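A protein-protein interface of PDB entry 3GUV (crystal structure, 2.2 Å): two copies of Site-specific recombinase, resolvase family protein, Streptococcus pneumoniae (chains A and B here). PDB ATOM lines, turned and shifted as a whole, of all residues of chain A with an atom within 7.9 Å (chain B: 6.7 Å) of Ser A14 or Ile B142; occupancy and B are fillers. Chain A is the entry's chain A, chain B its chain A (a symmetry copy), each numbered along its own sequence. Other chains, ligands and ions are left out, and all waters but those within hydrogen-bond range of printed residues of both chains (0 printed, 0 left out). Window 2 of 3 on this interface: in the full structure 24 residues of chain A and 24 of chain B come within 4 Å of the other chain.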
ATOM      1  N   ARG A  12      20.181 -18.288  29.110  1.00  0.00           N
ATOM      2  CA  ARG A  12      20.666 -17.790  27.792  1.00  0.00           C
ATOM      3  C   ARG A  12      19.570 -17.867  26.734  1.00  0.00           C
ATOM      4  O   ARG A  12      18.535 -18.470  26.957  1.00  0.00           O
ATOM      5  CB  ARG A  12      21.910 -18.567  27.315  1.00  0.00           C
ATOM      6  CG  ARG A  12      21.623 -20.103  27.160  1.00  0.00           C
ATOM      7  CD  ARG A  12      22.745 -20.878  26.510  1.00  0.00           C
ATOM      8  NE  ARG A  12      22.971 -20.389  25.158  1.00  0.00           N
ATOM      9  CZ  ARG A  12      24.013 -19.666  24.745  1.00  0.00           C
ATOM     10  NH1 ARG A  12      24.070 -19.273  23.468  1.00  0.00           N
ATOM     11  NH2 ARG A  12      25.000 -19.313  25.571  1.00  0.00           N
ATOM     12  N   VAL A  13      19.795 -17.234  25.599  1.00  0.00           N
ATOM     13  CA  VAL A  13      19.023 -17.461  24.374  1.00  0.00           C
ATOM     14  C   VAL A  13      19.975 -18.208  23.431  1.00  0.00           C
ATOM     15  O   VAL A  13      21.181 -18.175  23.633  1.00  0.00           O
ATOM     16  CB  VAL A  13      18.588 -16.158  23.695  1.00  0.00           C
ATOM     17  CG1 VAL A  13      17.756 -15.294  24.672  1.00  0.00           C
ATOM     18  CG2 VAL A  13      19.801 -15.378  23.211  1.00  0.00           C
ATOM     19  N   SER A  14      19.417 -18.889  22.434  1.00  0.00           N
ATOM     20  CA  SER A  14      20.174 -19.547  21.377  1.00  0.00           C
ATOM     21  C   SER A  14      20.525 -18.585  20.273  1.00  0.00           C
ATOM     22  O   SER A  14      21.618 -18.664  19.730  1.00  0.00           O
ATOM     23  CB  SER A  14      19.348 -20.658  20.724  1.00  0.00           C
ATOM     24  OG  SER A  14      18.840 -21.546  21.694  1.00  0.00           O
ATOM     25  N   THR A  15      19.566 -17.742  19.891  1.00  0.00           N
ATOM     26  CA  THR A  15      19.758 -16.792  18.772  1.00  0.00           C
ATOM     27  C   THR A  15      19.989 -15.417  19.346  1.00  0.00           C
ATOM     28  O   THR A  15      21.094 -15.162  19.783  1.00  0.00           O
ATOM     29  CB  THR A  15      18.581 -16.760  17.727  1.00  0.00           C
ATOM     30  OG1 THR A  15      17.329 -16.527  18.384  1.00  0.00           O
ATOM     31  CG2 THR A  15      18.528 -18.044  16.969  1.00  0.00           C
ATOM     32  N   SER A  16      18.955 -14.566  19.369  1.00  0.00           N
ATOM     33  CA  SER A  16      19.025 -13.204  19.946  1.00  0.00           C
ATOM     34  C   SER A  16      17.876 -12.887  20.916  1.00  0.00           C
ATOM     35  O   SER A  16      16.836 -13.562  20.905  1.00  0.00           O
ATOM     36  CB  SER A  16      19.108 -12.130  18.832  1.00  0.00           C
ATOM     37  OG  SER A  16      18.114 -12.311  17.840  1.00  0.00           O
ATOM     38  N   ILE A  17      18.072 -11.854  21.745  1.00  0.00           N
ATOM     39  CA  ILE A  17      17.050 -11.352  22.689  1.00  0.00           C
ATOM     40  C   ILE A  17      15.771 -10.829  22.011  1.00  0.00           C
ATOM     41  O   ILE A  17      14.659 -10.948  22.572  1.00  0.00           O
ATOM     42  CB  ILE A  17      17.608 -10.225  23.634  1.00  0.00           C
ATOM     43  CG1 ILE A  17      16.696 -10.063  24.871  1.00  0.00           C
ATOM     44  CG2 ILE A  17      17.759  -8.945  22.885  1.00  0.00           C
ATOM     45  CD1 ILE A  17      17.330  -9.324  26.102  1.00  0.00           C
ATOM     46  N   ILE A  19      14.376 -12.223  19.403  1.00  0.00           N
ATOM     47  CA  ILE A  19      13.572 -13.379  19.011  1.00  0.00           C
ATOM     48  C   ILE A  19      13.110 -14.184  20.224  1.00  0.00           C
ATOM     49  O   ILE A  19      11.992 -14.685  20.261  1.00  0.00           O
ATOM     50  CB  ILE A  19      14.401 -14.279  18.033  1.00  0.00           C
ATOM     51  CG1 ILE A  19      14.846 -13.460  16.808  1.00  0.00           C
ATOM     52  CG2 ILE A  19      13.655 -15.541  17.643  1.00  0.00           C
ATOM     53  CD1 ILE A  19      13.736 -12.537  16.195  1.00  0.00           C
ATOM     54  N   GLU A  20      13.983 -14.288  21.220  1.00  0.00           N
ATOM     55  CA  GLU A  20      13.810 -15.216  22.320  1.00  0.00           C
ATOM     56  C   GLU A  20      13.715 -14.580  23.714  1.00  0.00           C
ATOM     57  O   GLU A  20      13.349 -15.250  24.670  1.00  0.00           O
ATOM     58  CB  GLU A  20      14.996 -16.152  22.331  1.00  0.00           C
ATOM     59  CG  GLU A  20      14.949 -17.267  21.349  1.00  0.00           C
ATOM     60  CD  GLU A  20      16.157 -18.152  21.514  1.00  0.00           C
ATOM     61  OE1 GLU A  20      16.416 -18.621  22.662  1.00  0.00           O
ATOM     62  OE2 GLU A  20      16.861 -18.359  20.508  1.00  0.00           O
ATOM     63  N   GLY A  21      14.063 -13.301  23.828  1.00  0.00           N
ATOM     64  CA  GLY A  21      14.120 -12.577  25.100  1.00  0.00           C
ATOM     65  C   GLY A  21      12.876 -12.721  25.914  1.00  0.00           C
ATOM     66  O   GLY A  21      12.922 -12.964  27.146  1.00  0.00           O
ATOM     67  N   LEU A  24      12.652 -15.435  28.501  1.00  0.00           N
ATOM     68  CA  LEU A  24      13.759 -15.548  29.429  1.00  0.00           C
ATOM     69  C   LEU A  24      13.258 -15.328  30.806  1.00  0.00           C
ATOM     70  O   LEU A  24      13.659 -16.042  31.720  1.00  0.00           O
ATOM     71  CB  LEU A  24      14.865 -14.510  29.168  1.00  0.00           C
ATOM     72  CG  LEU A  24      16.026 -14.958  28.298  1.00  0.00           C
ATOM     73  CD1 LEU A  24      17.006 -13.771  28.037  1.00  0.00           C
ATOM     74  CD2 LEU A  24      16.729 -16.171  28.970  1.00  0.00           C
ATOM     75  N   ASP A  48      23.611 -15.135  29.309  1.00  0.00           N
ATOM     76  CA  ASP A  48      24.024 -14.741  27.948  1.00  0.00           C
ATOM     77  C   ASP A  48      22.742 -14.373  27.153  1.00  0.00           C
ATOM     78  O   ASP A  48      22.117 -15.247  26.540  1.00  0.00           O
ATOM     79  CB  ASP A  48      24.751 -15.906  27.298  1.00  0.00           C
ATOM     80  CG  ASP A  48      26.128 -16.141  27.896  1.00  0.00           C
ATOM     81  OD1 ASP A  48      26.930 -15.189  27.835  1.00  0.00           O
ATOM     82  OD2 ASP A  48      26.405 -17.264  28.406  1.00  0.00           O
ATOM     83  N   ALA A  49      22.317 -13.118  27.213  1.00  0.00           N
ATOM     84  CA  ALA A  49      20.909 -12.781  26.871  1.00  0.00           C
ATOM     85  C   ALA A  49      20.706 -12.423  25.414  1.00  0.00           C
ATOM     86  O   ALA A  49      19.563 -12.242  24.978  1.00  0.00           O
ATOM     87  CB  ALA A  49      20.337 -11.688  27.783  1.00  0.00           C
ATOM     88  N   GLY A  50      21.797 -12.359  24.648  1.00  0.00           N
ATOM     89  CA  GLY A  50      21.706 -12.195  23.204  1.00  0.00           C
ATOM     90  C   GLY A  50      21.424 -10.751  22.909  1.00  0.00           C
ATOM     91  O   GLY A  50      20.623 -10.455  22.017  1.00  0.00           O
ATOM     92  N   LYS A  54      24.824  -9.684  16.922  1.00  0.00           N
ATOM     93  CA  LYS A  54      25.017 -10.877  16.080  1.00  0.00           C
ATOM     94  C   LYS A  54      23.825 -11.890  16.104  1.00  0.00           C
ATOM     95  O   LYS A  54      22.943 -11.863  16.999  1.00  0.00           O
ATOM     96  CB  LYS A  54      26.363 -11.560  16.426  1.00  0.00           C
ATOM     97  CG  LYS A  54      26.483 -12.186  17.842  1.00  0.00           C
ATOM     98  CD  LYS A  54      27.961 -12.300  18.271  1.00  0.00           C
ATOM     99  CE  LYS A  54      28.307 -13.586  19.053  1.00  0.00           C
ATOM    100  NZ  LYS A  54      28.330 -13.413  20.545  1.00  0.00           N
ATOM    101  N   SER A  55      23.830 -12.772  15.093  1.00  0.00           N
ATOM    102  CA  SER A  55      22.732 -13.716  14.826  1.00  0.00           C
ATOM    103  C   SER A  55      22.558 -14.748  15.947  1.00  0.00           C
ATOM    104  O   SER A  55      21.445 -14.931  16.434  1.00  0.00           O
ATOM    105  CB  SER A  55      22.948 -14.432  13.484  1.00  0.00           C
ATOM    106  N   ILE A  56      23.655 -15.409  16.333  1.00  0.00           N
ATOM    107  CA  ILE A  56      23.651 -16.456  17.364  1.00  0.00           C
ATOM    108  C   ILE A  56      24.390 -15.965  18.631  1.00  0.00           C
ATOM    109  O   ILE A  56      25.427 -15.298  18.544  1.00  0.00           O
ATOM    110  CB  ILE A  56      24.275 -17.793  16.824  1.00  0.00           C
ATOM    111  CG1 ILE A  56      23.774 -18.102  15.389  1.00  0.00           C
ATOM    112  CG2 ILE A  56      23.978 -18.965  17.763  1.00  0.00           C
ATOM    113  CD1 ILE A  56      22.252 -18.091  15.234  1.00  0.00           C
ATOM    114  N   GLU A  57      23.845 -16.281  19.807  1.00  0.00           N
ATOM    115  CA  GLU A  57      24.419 -15.762  21.043  1.00  0.00           C
ATOM    116  C   GLU A  57      25.657 -16.559  21.442  1.00  0.00           C
ATOM    117  O   GLU A  57      25.740 -17.769  21.187  1.00  0.00           O
ATOM    118  CB  GLU A  57      23.403 -15.747  22.187  1.00  0.00           C
ATOM    119  CG  GLU A  57      23.931 -15.230  23.538  1.00  0.00           C
ATOM    120  CD  GLU A  57      24.461 -13.778  23.487  1.00  0.00           C
ATOM    121  OE1 GLU A  57      24.515 -13.078  24.544  1.00  0.00           O
ATOM    122  OE2 GLU A  57      24.810 -13.316  22.374  1.00  0.00           O
ATOM    123  N   GLY A  58      26.609 -15.856  22.064  1.00  0.00           N
ATOM    124  CA  GLY A  58      27.851 -16.440  22.547  1.00  0.00           C
ATOM    125  C   GLY A  58      27.751 -17.041  23.942  1.00  0.00           C
ATOM    126  O   GLY A  58      26.682 -17.565  24.366  1.00  0.00           O
ATOM    127  N   LYS A  83      16.800 -25.926  30.775  1.00  0.00           N
ATOM    128  CA  LYS A  83      16.952 -27.249  30.154  1.00  0.00           C
ATOM    129  C   LYS A  83      18.311 -27.321  29.432  1.00  0.00           C
ATOM    130  O   LYS A  83      18.969 -26.283  29.236  1.00  0.00           O
ATOM    131  CB  LYS A  83      15.788 -27.485  29.197  1.00  0.00           C
ATOM    132  CG  LYS A  83      15.674 -26.441  28.166  1.00  0.00           C
ATOM    133  CD  LYS A  83      14.363 -26.525  27.415  1.00  0.00           C
ATOM    134  CE  LYS A  83      14.295 -25.293  26.506  1.00  0.00           C
ATOM    135  NZ  LYS A  83      13.225 -25.365  25.468  1.00  0.00           N
ATOM    136  N   SER A  85      19.329 -27.781  26.307  1.00  0.00           N
ATOM    137  CA  SER A  85      19.445 -26.917  25.144  1.00  0.00           C
ATOM    138  C   SER A  85      19.540 -25.425  25.507  1.00  0.00           C
ATOM    139  O   SER A  85      19.577 -24.594  24.617  1.00  0.00           O
ATOM    140  CB  SER A  85      18.245 -27.109  24.243  1.00  0.00           C
ATOM    141  OG  SER A  85      17.073 -26.816  24.970  1.00  0.00           O
ATOM    142  N   ARG A  86      19.508 -25.085  26.793  1.00  0.00           N
ATOM    143  CA  ARG A  86      19.725 -23.700  27.224  1.00  0.00           C
ATOM    144  C   ARG A  86      20.930 -23.718  28.149  1.00  0.00           C
ATOM    145  O   ARG A  86      20.926 -23.128  29.251  1.00  0.00           O
ATOM    146  CB  ARG A  86      18.477 -23.138  27.898  1.00  0.00           C
ATOM    147  CG  ARG A  86      17.340 -22.862  26.934  1.00  0.00           C
ATOM    148  CD  ARG A  86      17.748 -21.773  25.948  1.00  0.00           C
ATOM    149  NE  ARG A  86      16.646 -21.364  25.103  1.00  0.00           N
ATOM    150  CZ  ARG A  86      16.168 -22.073  24.083  1.00  0.00           C
ATOM    151  NH1 ARG A  86      16.659 -23.267  23.777  1.00  0.00           N
ATOM    152  NH2 ARG A  86      15.166 -21.596  23.374  1.00  0.00           N
ATOM    153  N   PHE A  87      21.972 -24.399  27.639  1.00  0.00           N
ATOM    154  CA  PHE A  87      23.161 -24.719  28.393  1.00  0.00           C
ATOM    155  C   PHE A  87      24.287 -25.180  27.468  1.00  0.00           C
ATOM    156  O   PHE A  87      25.388 -24.679  27.564  1.00  0.00           O
ATOM    157  CB  PHE A  87      22.817 -25.772  29.447  1.00  0.00           C
ATOM    158  CG  PHE A  87      24.004 -26.320  30.167  1.00  0.00           C
ATOM    159  CD1 PHE A  87      24.754 -25.515  31.013  1.00  0.00           C
ATOM    160  CD2 PHE A  87      24.359 -27.639  30.022  1.00  0.00           C
ATOM    161  CE1 PHE A  87      25.847 -26.010  31.696  1.00  0.00           C
ATOM    162  CE2 PHE A  87      25.467 -28.149  30.688  1.00  0.00           C
ATOM    163  CZ  PHE A  87      26.215 -27.321  31.539  1.00  0.00           C
ATOM    164  N   ALA A  88      24.020 -26.155  26.596  1.00  0.00           N
ATOM    165  CA  ALA A  88      25.055 -26.731  25.710  1.00  0.00           C
ATOM    166  C   ALA A  88      24.597 -26.721  24.257  1.00  0.00           C
ATOM    167  O   ALA A  88      23.413 -26.557  23.965  1.00  0.00           O
ATOM    168  CB  ALA A  88      25.391 -28.148  26.152  1.00  0.00           C
ATOM    169  N   ARG B 137      17.227 -30.830  17.472  1.00  0.00           N
ATOM    170  CA  ARG B 137      16.080 -30.211  16.793  1.00  0.00           C
ATOM    171  C   ARG B 137      16.284 -28.705  16.667  1.00  0.00           C
ATOM    172  O   ARG B 137      16.092 -28.156  15.607  1.00  0.00           O
ATOM    173  CB  ARG B 137      14.759 -30.467  17.527  1.00  0.00           C
ATOM    174  CG  ARG B 137      14.203 -31.891  17.369  1.00  0.00           C
ATOM    175  CD  ARG B 137      12.720 -31.973  17.816  1.00  0.00           C
ATOM    176  NE  ARG B 137      12.607 -32.246  19.244  1.00  0.00           N
ATOM    177  CZ  ARG B 137      12.766 -33.451  19.791  1.00  0.00           C
ATOM    178  NH1 ARG B 137      13.040 -34.519  19.030  1.00  0.00           N
ATOM    179  NH2 ARG B 137      12.652 -33.596  21.108  1.00  0.00           N
ATOM    180  N   GLU B 138      16.708 -28.069  17.751  1.00  0.00           N
ATOM    181  CA  GLU B 138      16.938 -26.646  17.756  1.00  0.00           C
ATOM    182  C   GLU B 138      18.107 -26.216  16.871  1.00  0.00           C
ATOM    183  O   GLU B 138      18.021 -25.209  16.201  1.00  0.00           O
ATOM    184  CB  GLU B 138      17.187 -26.143  19.158  1.00  0.00           C
ATOM    185  CG  GLU B 138      17.022 -24.678  19.214  1.00  0.00           C
ATOM    186  CD  GLU B 138      16.932 -24.158  20.599  1.00  0.00           C
ATOM    187  OE1 GLU B 138      17.366 -24.862  21.549  1.00  0.00           O
ATOM    188  OE2 GLU B 138      16.425 -23.031  20.730  1.00  0.00           O
ATOM    189  N   ASN B 139      19.195 -26.975  16.856  1.00  0.00           N
ATOM    190  CA  ASN B 139      20.202 -26.784  15.834  1.00  0.00           C
ATOM    191  C   ASN B 139      19.655 -26.811  14.406  1.00  0.00           C
ATOM    192  O   ASN B 139      20.086 -26.021  13.576  1.00  0.00           O
ATOM    193  CB  ASN B 139      21.342 -27.783  16.000  1.00  0.00           C
ATOM    194  CG  ASN B 139      22.219 -27.440  17.175  1.00  0.00           C
ATOM    195  OD1 ASN B 139      22.201 -26.309  17.658  1.00  0.00           O
ATOM    196  ND2 ASN B 139      22.976 -28.403  17.651  1.00  0.00           N
ATOM    197  N   ILE B 140      18.713 -27.696  14.125  1.00  0.00           N
ATOM    198  CA  ILE B 140      18.089 -27.791  12.785  1.00  0.00           C
ATOM    199  C   ILE B 140      17.240 -26.540  12.472  1.00  0.00           C
ATOM    200  O   ILE B 140      17.351 -25.972  11.376  1.00  0.00           O
ATOM    201  CB  ILE B 140      17.251 -29.116  12.610  1.00  0.00           C
ATOM    202  CG1 ILE B 140      18.177 -30.341  12.396  1.00  0.00           C
ATOM    203  CG2 ILE B 140      16.239 -29.000  11.457  1.00  0.00           C
ATOM    204  CD1 ILE B 140      18.840 -30.414  11.020  1.00  0.00           C
ATOM    205  N   ARG B 141      16.393 -26.129  13.418  1.00  0.00           N
ATOM    206  CA  ARG B 141      15.632 -24.851  13.300  1.00  0.00           C
ATOM    207  C   ARG B 141      16.554 -23.622  13.026  1.00  0.00           C
ATOM    208  O   ARG B 141      16.251 -22.781  12.182  1.00  0.00           O
ATOM    209  CB  ARG B 141      14.752 -24.611  14.558  1.00  0.00           C
ATOM    210  CG  ARG B 141      13.648 -25.702  14.756  1.00  0.00           C
ATOM    211  CD  ARG B 141      12.581 -25.369  15.808  1.00  0.00           C
ATOM    212  NE  ARG B 141      13.126 -25.399  17.171  1.00  0.00           N
ATOM    213  CZ  ARG B 141      12.975 -26.385  18.070  1.00  0.00           C
ATOM    214  NH1 ARG B 141      12.260 -27.477  17.808  1.00  0.00           N
ATOM    215  NH2 ARG B 141      13.547 -26.268  19.266  1.00  0.00           N
ATOM    216  N   ILE B 142      17.667 -23.530  13.750  1.00  0.00           N
ATOM    217  CA  ILE B 142      18.620 -22.426  13.572  1.00  0.00           C
ATOM    218  C   ILE B 142      19.246 -22.456  12.168  1.00  0.00           C
ATOM    219  O   ILE B 142      19.340 -21.407  11.503  1.00  0.00           O
ATOM    220  CB  ILE B 142      19.726 -22.435  14.674  1.00  0.00           C
ATOM    221  CG1 ILE B 142      19.130 -22.028  16.023  1.00  0.00           C
ATOM    222  CG2 ILE B 142      20.903 -21.545  14.295  1.00  0.00           C
ATOM    223  CD1 ILE B 142      20.103 -22.160  17.178  1.00  0.00           C
ATOM    224  N   GLN B 143      19.627 -23.649  11.702  1.00  0.00           N
ATOM    225  CA  GLN B 143      20.148 -23.787  10.331  1.00  0.00           C
ATOM    226  C   GLN B 143      19.080 -23.414   9.285  1.00  0.00           C
ATOM    227  O   GLN B 143      19.381 -22.736   8.313  1.00  0.00           O
ATOM    228  CB  GLN B 143      20.663 -25.203  10.065  1.00  0.00           C
ATOM    229  CG  GLN B 143      21.867 -25.593  10.916  1.00  0.00           C
ATOM    230  CD  GLN B 143      22.151 -27.106  10.928  1.00  0.00           C
ATOM    231  OE1 GLN B 143      21.578 -27.869  10.134  1.00  0.00           O
ATOM    232  NE2 GLN B 143      23.038 -27.543  11.839  1.00  0.00           N
ATOM    233  N   THR B 144      17.842 -23.861   9.480  1.00  0.00           N
ATOM    234  CA  THR B 144      16.752 -23.491   8.558  1.00  0.00           C
ATOM    235  C   THR B 144      16.518 -21.967   8.574  1.00  0.00           C
ATOM    236  O   THR B 144      16.386 -21.367   7.529  1.00  0.00           O
ATOM    237  CB  THR B 144      15.413 -24.210   8.861  1.00  0.00           C
ATOM    238  OG1 THR B 144      15.617 -25.629   8.973  1.00  0.00           O
ATOM    239  CG2 THR B 144      14.397 -23.930   7.757  1.00  0.00           C
ATOM    240  N   MET B 145      16.513 -21.359   9.759  1.00  0.00           N
ATOM    241  CA  MET B 145      16.343 -19.921   9.869  1.00  0.00           C
ATOM    242  C   MET B 145      17.473 -19.145   9.139  1.00  0.00           C
ATOM    243  O   MET B 145      17.193 -18.205   8.376  1.00  0.00           O
ATOM    244  CB  MET B 145      16.239 -19.508  11.335  1.00  0.00           C
ATOM    245  CG  MET B 145      15.792 -18.036  11.595  1.00  0.00           C
ATOM    246  SD  MET B 145      15.731 -17.660  13.377  1.00  0.00           S
ATOM    247  CE  MET B 145      15.151 -19.303  13.891  1.00  0.00           C
ATOM    248  N   GLU B 146      18.731 -19.544   9.363  1.00  0.00           N
ATOM    249  CA  GLU B 146      19.880 -18.948   8.660  1.00  0.00           C
ATOM    250  C   GLU B 146      19.769 -19.138   7.168  1.00  0.00           C
ATOM    251  O   GLU B 146      20.008 -18.201   6.417  1.00  0.00           O
ATOM    252  CB  GLU B 146      21.208 -19.518   9.153  1.00  0.00           C
ATOM    253  CG  GLU B 146      21.688 -18.908  10.467  1.00  0.00           C
ATOM    254  CD  GLU B 146      22.271 -17.477  10.344  1.00  0.00           C
ATOM    255  OE1 GLU B 146      23.222 -17.188  11.129  1.00  0.00           O
ATOM    256  OE2 GLU B 146      21.801 -16.647   9.501  1.00  0.00           O
ATOM    257  N   GLY B 147      19.376 -20.331   6.733  1.00  0.00           N
ATOM    258  CA  GLY B 147      19.081 -20.575   5.313  1.00  0.00           C
ATOM    259  C   GLY B 147      17.966 -19.707   4.710  1.00  0.00           C
ATOM    260  O   GLY B 147      18.049 -19.324   3.525  1.00  0.00           O
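The side-chain carboxylate (OE2) of Glu B138 sits at hydrogen-bond distance from the side-chain hydroxyl (OG) of Ser A14 (3.0 Å). The guanidinium group (NH1) of Arg A86 lies within salt-bridge range of the side-chain carboxylate (OE1) of Glu B138, 2.8 Å away.
The side-chain carboxylate (OE1) of Glu A20 lies within hydrogen-bond range of the backbone NH (N) of Ser A14. The backbone NH (N) of Glu A57 lies within hydrogen-bond range of the backbone carbonyl oxygen (O) of Ser A14, at 3.3 Å. The side-chain hydroxyl (OG) of Ser A14 lies within hydrogen-bond range of the guanidinium group (NH1) of Arg A86 (3.5 Å). OE1 of Glu A20 is in salt-bridge range of NH2 of Arg A86 (3.3 Å).
Ser A14 touches Ile B142. Ser A55 touches Glu B146. CD1 of Ile A56 touches CG2 of Ile B142, 3.8 Å away. Ser A85 touches Glu B138.
Of the printed residues of chain B, Ser A55 touches Glu B146 (3.6 Å). Of the printed residues of chain B, Arg A86 touches Glu B138. Arg B137 touches none of the printed residues of chain A. Printed residues of chain A within 4 Å of Glu B138: Ser A14 (3.0 Å), Ser A85 (3.6 Å) and Arg A86 (2.8 Å). Printed residues of chain A within 4 Å of Glu B146: Ser A55 (3.6 Å).
Of the 23 printed residues of chain A, 5 touch a printed residue of chain B. Among the printed residues, 6 pairs touch across the chains.
No position is printed for both chains.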
